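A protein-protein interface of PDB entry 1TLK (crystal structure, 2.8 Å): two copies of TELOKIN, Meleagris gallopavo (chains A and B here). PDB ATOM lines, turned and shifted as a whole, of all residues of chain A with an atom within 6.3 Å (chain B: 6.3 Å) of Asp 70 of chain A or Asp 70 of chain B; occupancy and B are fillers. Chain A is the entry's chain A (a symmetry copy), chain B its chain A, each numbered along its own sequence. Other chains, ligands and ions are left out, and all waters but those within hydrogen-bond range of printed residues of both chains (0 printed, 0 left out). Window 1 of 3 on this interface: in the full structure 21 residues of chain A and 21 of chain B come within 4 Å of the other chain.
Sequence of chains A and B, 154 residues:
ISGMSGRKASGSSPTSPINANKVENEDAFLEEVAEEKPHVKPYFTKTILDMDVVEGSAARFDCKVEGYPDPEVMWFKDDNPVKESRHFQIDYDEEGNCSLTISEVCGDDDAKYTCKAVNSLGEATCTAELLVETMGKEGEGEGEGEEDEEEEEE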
ATOM      1  N   LYS A  37       1.945 -15.630  -2.443  1.00  0.00           N
ATOM      2  CA  LYS A  37       0.998 -15.949  -1.386  1.00  0.00           C
ATOM      3  C   LYS A  37       0.899 -17.446  -1.162  1.00  0.00           C
ATOM      4  O   LYS A  37       1.223 -18.243  -2.032  1.00  0.00           O
ATOM      5  CB  LYS A  37      -0.383 -15.406  -1.670  1.00  0.00           C
ATOM      6  CG  LYS A  37      -0.576 -14.012  -1.117  1.00  0.00           C
ATOM      7  CD  LYS A  37      -1.565 -13.189  -1.933  1.00  0.00           C
ATOM      8  CE  LYS A  37      -2.630 -12.607  -1.017  1.00  0.00           C
ATOM      9  NZ  LYS A  37      -3.292 -11.359  -1.579  1.00  0.00           N
ATOM     10  N   GLY A  67      -8.786 -16.139   0.808  1.00  0.00           N
ATOM     11  CA  GLY A  67      -8.445 -17.319   0.033  1.00  0.00           C
ATOM     12  C   GLY A  67      -7.528 -16.969  -1.119  1.00  0.00           C
ATOM     13  O   GLY A  67      -7.480 -15.810  -1.567  1.00  0.00           O
ATOM     14  N   TYR A  68      -6.837 -18.002  -1.628  1.00  0.00           N
ATOM     15  CA  TYR A  68      -5.876 -17.918  -2.722  1.00  0.00           C
ATOM     16  C   TYR A  68      -5.509 -19.241  -3.367  1.00  0.00           C
ATOM     17  O   TYR A  68      -5.100 -20.172  -2.676  1.00  0.00           O
ATOM     18  CB  TYR A  68      -4.519 -17.518  -2.144  1.00  0.00           C
ATOM     19  CG  TYR A  68      -3.532 -17.361  -3.263  1.00  0.00           C
ATOM     20  CD1 TYR A  68      -3.700 -16.256  -4.099  1.00  0.00           C
ATOM     21  CD2 TYR A  68      -2.439 -18.211  -3.458  1.00  0.00           C
ATOM     22  CE1 TYR A  68      -2.839 -16.052  -5.176  1.00  0.00           C
ATOM     23  CE2 TYR A  68      -1.521 -17.941  -4.475  1.00  0.00           C
ATOM     24  CZ  TYR A  68      -1.747 -16.896  -5.366  1.00  0.00           C
ATOM     25  OH  TYR A  68      -0.863 -16.675  -6.390  1.00  0.00           O
ATOM     26  N   PRO A  69      -5.551 -19.316  -4.690  1.00  0.00           N
ATOM     27  CA  PRO A  69      -6.016 -18.276  -5.564  1.00  0.00           C
ATOM     28  C   PRO A  69      -7.382 -17.807  -5.222  1.00  0.00           C
ATOM     29  O   PRO A  69      -8.288 -18.565  -4.878  1.00  0.00           O
ATOM     30  CB  PRO A  69      -6.061 -18.828  -6.981  1.00  0.00           C
ATOM     31  CG  PRO A  69      -5.560 -20.260  -6.889  1.00  0.00           C
ATOM     32  CD  PRO A  69      -5.224 -20.552  -5.433  1.00  0.00           C
ATOM     33  N   ASP A  70      -7.460 -16.505  -5.355  1.00  0.00           N
ATOM     34  CA  ASP A  70      -8.669 -15.801  -5.107  1.00  0.00           C
ATOM     35  C   ASP A  70      -9.848 -16.566  -5.705  1.00  0.00           C
ATOM     36  O   ASP A  70      -9.863 -16.868  -6.897  1.00  0.00           O
ATOM     37  CB  ASP A  70      -8.557 -14.371  -5.684  1.00  0.00           C
ATOM     38  CG  ASP A  70      -7.345 -13.626  -5.194  1.00  0.00           C
ATOM     39  OD1 ASP A  70      -6.214 -14.149  -5.603  1.00  0.00           O
ATOM     40  OD2 ASP A  70      -7.416 -12.631  -4.492  1.00  0.00           O
ATOM     41  N   PRO A  71     -10.815 -16.888  -4.832  1.00  0.00           N
ATOM     42  CA  PRO A  71     -12.077 -17.558  -5.127  1.00  0.00           C
ATOM     43  C   PRO A  71     -12.982 -16.889  -6.127  1.00  0.00           C
ATOM     44  O   PRO A  71     -12.836 -15.721  -6.464  1.00  0.00           O
ATOM     45  CB  PRO A  71     -12.885 -17.572  -3.822  1.00  0.00           C
ATOM     46  CG  PRO A  71     -11.968 -17.063  -2.723  1.00  0.00           C
ATOM     47  CD  PRO A  71     -10.706 -16.536  -3.392  1.00  0.00           C
ATOM     48  N   GLU A  72     -13.946 -17.666  -6.572  1.00  0.00           N
ATOM     49  CA  GLU A  72     -14.904 -17.112  -7.459  1.00  0.00           C
ATOM     50  C   GLU A  72     -16.137 -17.096  -6.659  1.00  0.00           C
ATOM     51  O   GLU A  72     -16.405 -17.940  -5.800  1.00  0.00           O
ATOM     52  CB  GLU A  72     -15.180 -17.860  -8.733  1.00  0.00           C
ATOM     53  CG  GLU A  72     -13.991 -17.771  -9.670  1.00  0.00           C
ATOM     54  CD  GLU A  72     -14.249 -18.720 -10.781  1.00  0.00           C
ATOM     55  OE1 GLU A  72     -14.641 -19.899 -10.358  1.00  0.00           O
ATOM     56  OE2 GLU A  72     -14.150 -18.414 -11.952  1.00  0.00           O
ATOM     57  N   TYR A  92     -17.449  -6.975  -6.168  1.00  0.00           N
ATOM     58  CA  TYR A  92     -16.472  -7.822  -5.531  1.00  0.00           C
ATOM     59  C   TYR A  92     -15.063  -7.226  -5.579  1.00  0.00           C
ATOM     60  O   TYR A  92     -14.421  -7.269  -6.620  1.00  0.00           O
ATOM     61  CB  TYR A  92     -16.568  -9.099  -6.371  1.00  0.00           C
ATOM     62  CG  TYR A  92     -15.685 -10.178  -5.868  1.00  0.00           C
ATOM     63  CD1 TYR A  92     -15.325 -10.209  -4.524  1.00  0.00           C
ATOM     64  CD2 TYR A  92     -15.260 -11.185  -6.727  1.00  0.00           C
ATOM     65  CE1 TYR A  92     -14.513 -11.239  -4.060  1.00  0.00           C
ATOM     66  CE2 TYR A  92     -14.408 -12.196  -6.285  1.00  0.00           C
ATOM     67  CZ  TYR A  92     -14.042 -12.220  -4.940  1.00  0.00           C
ATOM     68  OH  TYR A  92     -13.237 -13.223  -4.470  1.00  0.00           O
ATOM     69  N   GLU A  94     -10.983  -6.219  -4.688  1.00  0.00           N
ATOM     70  CA  GLU A  94      -9.710  -6.845  -4.738  1.00  0.00           C
ATOM     71  C   GLU A  94      -9.464  -7.256  -3.287  1.00  0.00           C
ATOM     72  O   GLU A  94      -8.660  -8.137  -2.988  1.00  0.00           O
ATOM     73  CB  GLU A  94      -8.671  -5.771  -5.083  1.00  0.00           C
ATOM     74  CG  GLU A  94      -9.334  -4.538  -5.732  1.00  0.00           C
ATOM     75  CD  GLU A  94      -9.163  -3.275  -4.944  1.00  0.00           C
ATOM     76  OE1 GLU A  94      -8.341  -3.139  -4.056  1.00  0.00           O
ATOM     77  OE2 GLU A  94      -9.994  -2.330  -5.315  1.00  0.00           O
ATOM     78  N   VAL A 118     -15.438 -20.214  -4.357  1.00  0.00           N
ATOM     79  CA  VAL A 118     -14.725 -21.429  -4.667  1.00  0.00           C
ATOM     80  C   VAL A 118     -13.428 -21.119  -5.393  1.00  0.00           C
ATOM     81  O   VAL A 118     -13.333 -20.131  -6.115  1.00  0.00           O
ATOM     82  CB  VAL A 118     -15.551 -22.396  -5.519  1.00  0.00           C
ATOM     83  CG1 VAL A 118     -16.811 -22.849  -4.794  1.00  0.00           C
ATOM     84  CG2 VAL A 118     -15.912 -21.760  -6.857  1.00  0.00           C
ATOM     85  N   ASN A 119     -12.437 -21.985  -5.201  1.00  0.00           N
ATOM     86  CA  ASN A 119     -11.120 -21.927  -5.817  1.00  0.00           C
ATOM     87  C   ASN A 119     -10.623 -23.365  -5.882  1.00  0.00           C
ATOM     88  O   ASN A 119     -11.416 -24.274  -5.549  1.00  0.00           O
ATOM     89  CB  ASN A 119     -10.112 -21.011  -5.121  1.00  0.00           C
ATOM     90  CG  ASN A 119      -9.645 -21.657  -3.840  1.00  0.00           C
ATOM     91  OD1 ASN A 119     -10.323 -22.546  -3.314  1.00  0.00           O
ATOM     92  ND2 ASN A 119      -8.486 -21.236  -3.337  1.00  0.00           N
ATOM     93  N   LYS B  37     -12.314 -11.225  -9.124  1.00  0.00           N
ATOM     94  CA  LYS B  37     -11.823  -9.965  -8.590  1.00  0.00           C
ATOM     95  C   LYS B  37     -11.471  -8.990  -9.697  1.00  0.00           C
ATOM     96  O   LYS B  37     -11.222  -9.378 -10.832  1.00  0.00           O
ATOM     97  CB  LYS B  37     -10.615 -10.151  -7.702  1.00  0.00           C
ATOM     98  CG  LYS B  37     -10.993 -10.362  -6.253  1.00  0.00           C
ATOM     99  CD  LYS B  37      -9.986 -11.223  -5.502  1.00  0.00           C
ATOM    100  CE  LYS B  37      -9.546 -10.513  -4.233  1.00  0.00           C
ATOM    101  NZ  LYS B  37      -9.030 -11.459  -3.161  1.00  0.00           N
ATOM    102  N   GLY B  67      -3.988  -5.744  -3.966  1.00  0.00           N
ATOM    103  CA  GLY B  67      -3.702  -5.861  -5.385  1.00  0.00           C
ATOM    104  C   GLY B  67      -4.136  -7.209  -5.919  1.00  0.00           C
ATOM    105  O   GLY B  67      -4.274  -8.183  -5.159  1.00  0.00           O
ATOM    106  N   TYR B  68      -4.301  -7.264  -7.251  1.00  0.00           N
ATOM    107  CA  TYR B  68      -4.736  -8.437  -8.001  1.00  0.00           C
ATOM    108  C   TYR B  68      -4.490  -8.380  -9.497  1.00  0.00           C
ATOM    109  O   TYR B  68      -4.908  -7.430 -10.155  1.00  0.00           O
ATOM    110  CB  TYR B  68      -6.263  -8.485  -7.983  1.00  0.00           C
ATOM    111  CG  TYR B  68      -6.727  -9.723  -8.692  1.00  0.00           C
ATOM    112  CD1 TYR B  68      -6.505 -10.939  -8.045  1.00  0.00           C
ATOM    113  CD2 TYR B  68      -7.416  -9.708  -9.908  1.00  0.00           C
ATOM    114  CE1 TYR B  68      -6.885 -12.137  -8.648  1.00  0.00           C
ATOM    115  CE2 TYR B  68      -7.888 -10.902 -10.456  1.00  0.00           C
ATOM    116  CZ  TYR B  68      -7.578 -12.120  -9.857  1.00  0.00           C
ATOM    117  OH  TYR B  68      -8.004 -13.288 -10.435  1.00  0.00           O
ATOM    118  N   PRO B  69      -3.906  -9.424 -10.068  1.00  0.00           N
ATOM    119  CA  PRO B  69      -3.392 -10.569  -9.369  1.00  0.00           C
ATOM    120  C   PRO B  69      -2.429 -10.204  -8.301  1.00  0.00           C
ATOM    121  O   PRO B  69      -1.584  -9.318  -8.429  1.00  0.00           O
ATOM    122  CB  PRO B  69      -2.654 -11.447 -10.371  1.00  0.00           C
ATOM    123  CG  PRO B  69      -2.797 -10.756 -11.718  1.00  0.00           C
ATOM    124  CD  PRO B  69      -3.607  -9.483 -11.514  1.00  0.00           C
ATOM    125  N   ASP B  70      -2.614 -10.961  -7.247  1.00  0.00           N
ATOM    126  CA  ASP B  70      -1.808 -10.831  -6.083  1.00  0.00           C
ATOM    127  C   ASP B  70      -0.344 -10.655  -6.482  1.00  0.00           C
ATOM    128  O   ASP B  70       0.217 -11.482  -7.200  1.00  0.00           O
ATOM    129  CB  ASP B  70      -2.015 -12.066  -5.176  1.00  0.00           C
ATOM    130  CG  ASP B  70      -3.461 -12.328  -4.850  1.00  0.00           C
ATOM    131  OD1 ASP B  70      -4.175 -12.666  -5.897  1.00  0.00           O
ATOM    132  OD2 ASP B  70      -3.913 -12.241  -3.721  1.00  0.00           O
ATOM    133  N   PRO B  71       0.240  -9.541  -6.015  1.00  0.00           N
ATOM    134  CA  PRO B  71       1.633  -9.144  -6.181  1.00  0.00           C
ATOM    135  C   PRO B  71       2.676 -10.098  -5.665  1.00  0.00           C
ATOM    136  O   PRO B  71       2.406 -11.008  -4.891  1.00  0.00           O
ATOM    137  CB  PRO B  71       1.831  -7.868  -5.351  1.00  0.00           C
ATOM    138  CG  PRO B  71       0.458  -7.436  -4.861  1.00  0.00           C
ATOM    139  CD  PRO B  71      -0.516  -8.557  -5.195  1.00  0.00           C
ATOM    140  N   GLU B  72       3.891  -9.840  -6.098  1.00  0.00           N
ATOM    141  CA  GLU B  72       4.964 -10.631  -5.610  1.00  0.00           C
ATOM    142  C   GLU B  72       5.733  -9.686  -4.786  1.00  0.00           C
ATOM    143  O   GLU B  72       5.827  -8.482  -5.035  1.00  0.00           O
ATOM    144  CB  GLU B  72       5.893 -11.235  -6.624  1.00  0.00           C
ATOM    145  CG  GLU B  72       5.194 -12.336  -7.399  1.00  0.00           C
ATOM    146  CD  GLU B  72       6.091 -12.707  -8.520  1.00  0.00           C
ATOM    147  OE1 GLU B  72       6.547 -11.661  -9.169  1.00  0.00           O
ATOM    148  OE2 GLU B  72       6.398 -13.854  -8.773  1.00  0.00           O
ATOM    149  N   TYR B  92       4.308 -14.149   4.294  1.00  0.00           N
ATOM    150  CA  TYR B  92       3.387 -13.420   3.457  1.00  0.00           C
ATOM    151  C   TYR B  92       2.018 -14.097   3.368  1.00  0.00           C
ATOM    152  O   TYR B  92       1.875 -15.088   2.661  1.00  0.00           O
ATOM    153  CB  TYR B  92       4.110 -13.439   2.107  1.00  0.00           C
ATOM    154  CG  TYR B  92       3.382 -12.679   1.063  1.00  0.00           C
ATOM    155  CD1 TYR B  92       2.534 -11.638   1.427  1.00  0.00           C
ATOM    156  CD2 TYR B  92       3.586 -12.974  -0.281  1.00  0.00           C
ATOM    157  CE1 TYR B  92       1.872 -10.920   0.436  1.00  0.00           C
ATOM    158  CE2 TYR B  92       2.894 -12.293  -1.281  1.00  0.00           C
ATOM    159  CZ  TYR B  92       2.037 -11.256  -0.912  1.00  0.00           C
ATOM    160  OH  TYR B  92       1.374 -10.545  -1.875  1.00  0.00           O
ATOM    161  N   GLU B  94      -2.190 -14.840   2.923  1.00  0.00           N
ATOM    162  CA  GLU B  94      -3.149 -14.863   1.877  1.00  0.00           C
ATOM    163  C   GLU B  94      -3.850 -13.511   2.017  1.00  0.00           C
ATOM    164  O   GLU B  94      -4.473 -13.003   1.086  1.00  0.00           O
ATOM    165  CB  GLU B  94      -4.185 -15.942   2.213  1.00  0.00           C
ATOM    166  CG  GLU B  94      -3.630 -16.953   3.237  1.00  0.00           C
ATOM    167  CD  GLU B  94      -4.394 -16.988   4.526  1.00  0.00           C
ATOM    168  OE1 GLU B  94      -5.509 -16.518   4.662  1.00  0.00           O
ATOM    169  OE2 GLU B  94      -3.733 -17.582   5.492  1.00  0.00           O
ATOM    170  N   VAL B 118       4.930  -6.355  -6.727  1.00  0.00           N
ATOM    171  CA  VAL B 118       4.710  -6.157  -8.138  1.00  0.00           C
ATOM    172  C   VAL B 118       3.777  -7.222  -8.689  1.00  0.00           C
ATOM    173  O   VAL B 118       3.748  -8.346  -8.198  1.00  0.00           O
ATOM    174  CB  VAL B 118       6.010  -6.171  -8.946  1.00  0.00           C
ATOM    175  CG1 VAL B 118       6.943  -5.043  -8.528  1.00  0.00           C
ATOM    176  CG2 VAL B 118       6.715  -7.517  -8.808  1.00  0.00           C
ATOM    177  N   ASN B 119       3.028  -6.855  -9.725  1.00  0.00           N
ATOM    178  CA  ASN B 119       2.093  -7.705 -10.448  1.00  0.00           C
ATOM    179  C   ASN B 119       2.019  -7.140 -11.860  1.00  0.00           C
ATOM    180  O   ASN B 119       2.802  -6.213 -12.162  1.00  0.00           O
ATOM    181  CB  ASN B 119       0.706  -7.836  -9.817  1.00  0.00           C
ATOM    182  CG  ASN B 119      -0.067  -6.558 -10.028  1.00  0.00           C
ATOM    183  OD1 ASN B 119       0.533  -5.508 -10.282  1.00  0.00           O
ATOM    184  ND2 ASN B 119      -1.394  -6.632  -9.943  1.00  0.00           N
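Lys 37 of chain A touches Asp 70 of chain B, and with the chains exchanged Asp 70 of chain A touches Lys 37 of chain B.
Lys 37 of chain A touches Glu 94 of chain B, and with the chains exchanged Glu 94 of chain A touches Lys 37 of chain B.
Tyr 68 of chain A touches Asp 70 of chain B, and with the chains exchanged Asp 70 of chain A touches Tyr 68 of chain B.
Asp 70 of chain B touches its own counterpart, Asp 70 of chain A.
Of the 11 printed residues of chain B, 5 touch a printed residue of chain A.
Of the 11 printed residues of chain A, 5 touch a printed residue of chain B.
Printed residues of chain A that touch a printed residue of chain B: Lys 37, Tyr 68, Asp 70, Tyr 92 and Glu 94.
Hydrophobic or aromatic side chains of chain A that line the printed part of chain B: Tyr 68 and Tyr 92.
Among the printed residues, 9 pairs touch across the chains.
Among the printed residues, Asp or Glu carboxylates within 4 Å of a Lys or Arg side-chain nitrogen of the other chain: Lys 37 of chain A with Asp 70 of chain B and Asp 70 of chain A with Lys 37 of chain B.
Lys 37 of chain A touches Tyr 92 of chain B.
OD1 of Asp 70 of chain B touches CE1 of Tyr 68 of chain A, 3.7 Å away.
Tyr 68 of chain B touches Asp 70 of chain A (CE1 to OD1, 3.7 Å).
Tyr 92 of chain A touches Lys 37 of chain B (CE2 to N, 3.7 Å).
Asp 70 of chain A touches three residues of chain B.
Asp 70 of chain B touches just these residues of chain A: Lys 37, Tyr 68 and Asp 70.
Printed residues of chain A within 4 Å of Glu 94 of chain B: Lys 37 (2.8 Å).
Of the printed residues of chain B, Tyr 92 of chain A touches Lys 37 (3.7 Å).
Printed residues of chain B within 4 Å of Lys 37 of chain A: Asp 70 (2.4 Å), Tyr 92 (3.7 Å) and Glu 94 (2.8 Å).
Glu 72 of chain A touches none of the printed residues of chain B.
The nearest residue of chain B that does not touch Asp 70 of chain A is Gly 67 of chain B (5.5 Å).
The nearest residue of chain A that does not touch Asp 70 of chain B is Gly 67 of chain A (5.5 Å).
The side-chain amino group (NZ) of Lys 37 of chain B sits close to the backbone carbonyl oxygen (O) of Glu 94 of chain A (3.3 Å).
OD1 of Asp 70 of chain A sits close to OD1 of Asp 70 of chain B (2.5 Å).
O of Glu 94 of chain B sits close to NZ of Lys 37 of chain A (3.3 Å).
NZ of Lys 37 of chain A sits close to OD2 of Asp 70 of chain B (2.4 Å).
NZ of Lys 37 of chain B lies close to OD2 of Asp 70 of chain A (2.4 Å).
The backbone carbonyl oxygen of Pro 71 of chain B is in hydrogen-bond range of the side-chain hydroxyl of Tyr 92 of chain B (3.2 Å).
OH of Tyr 92 of chain A sits at hydrogen-bond distance from O of Pro 71 of chain A (3.2 Å).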
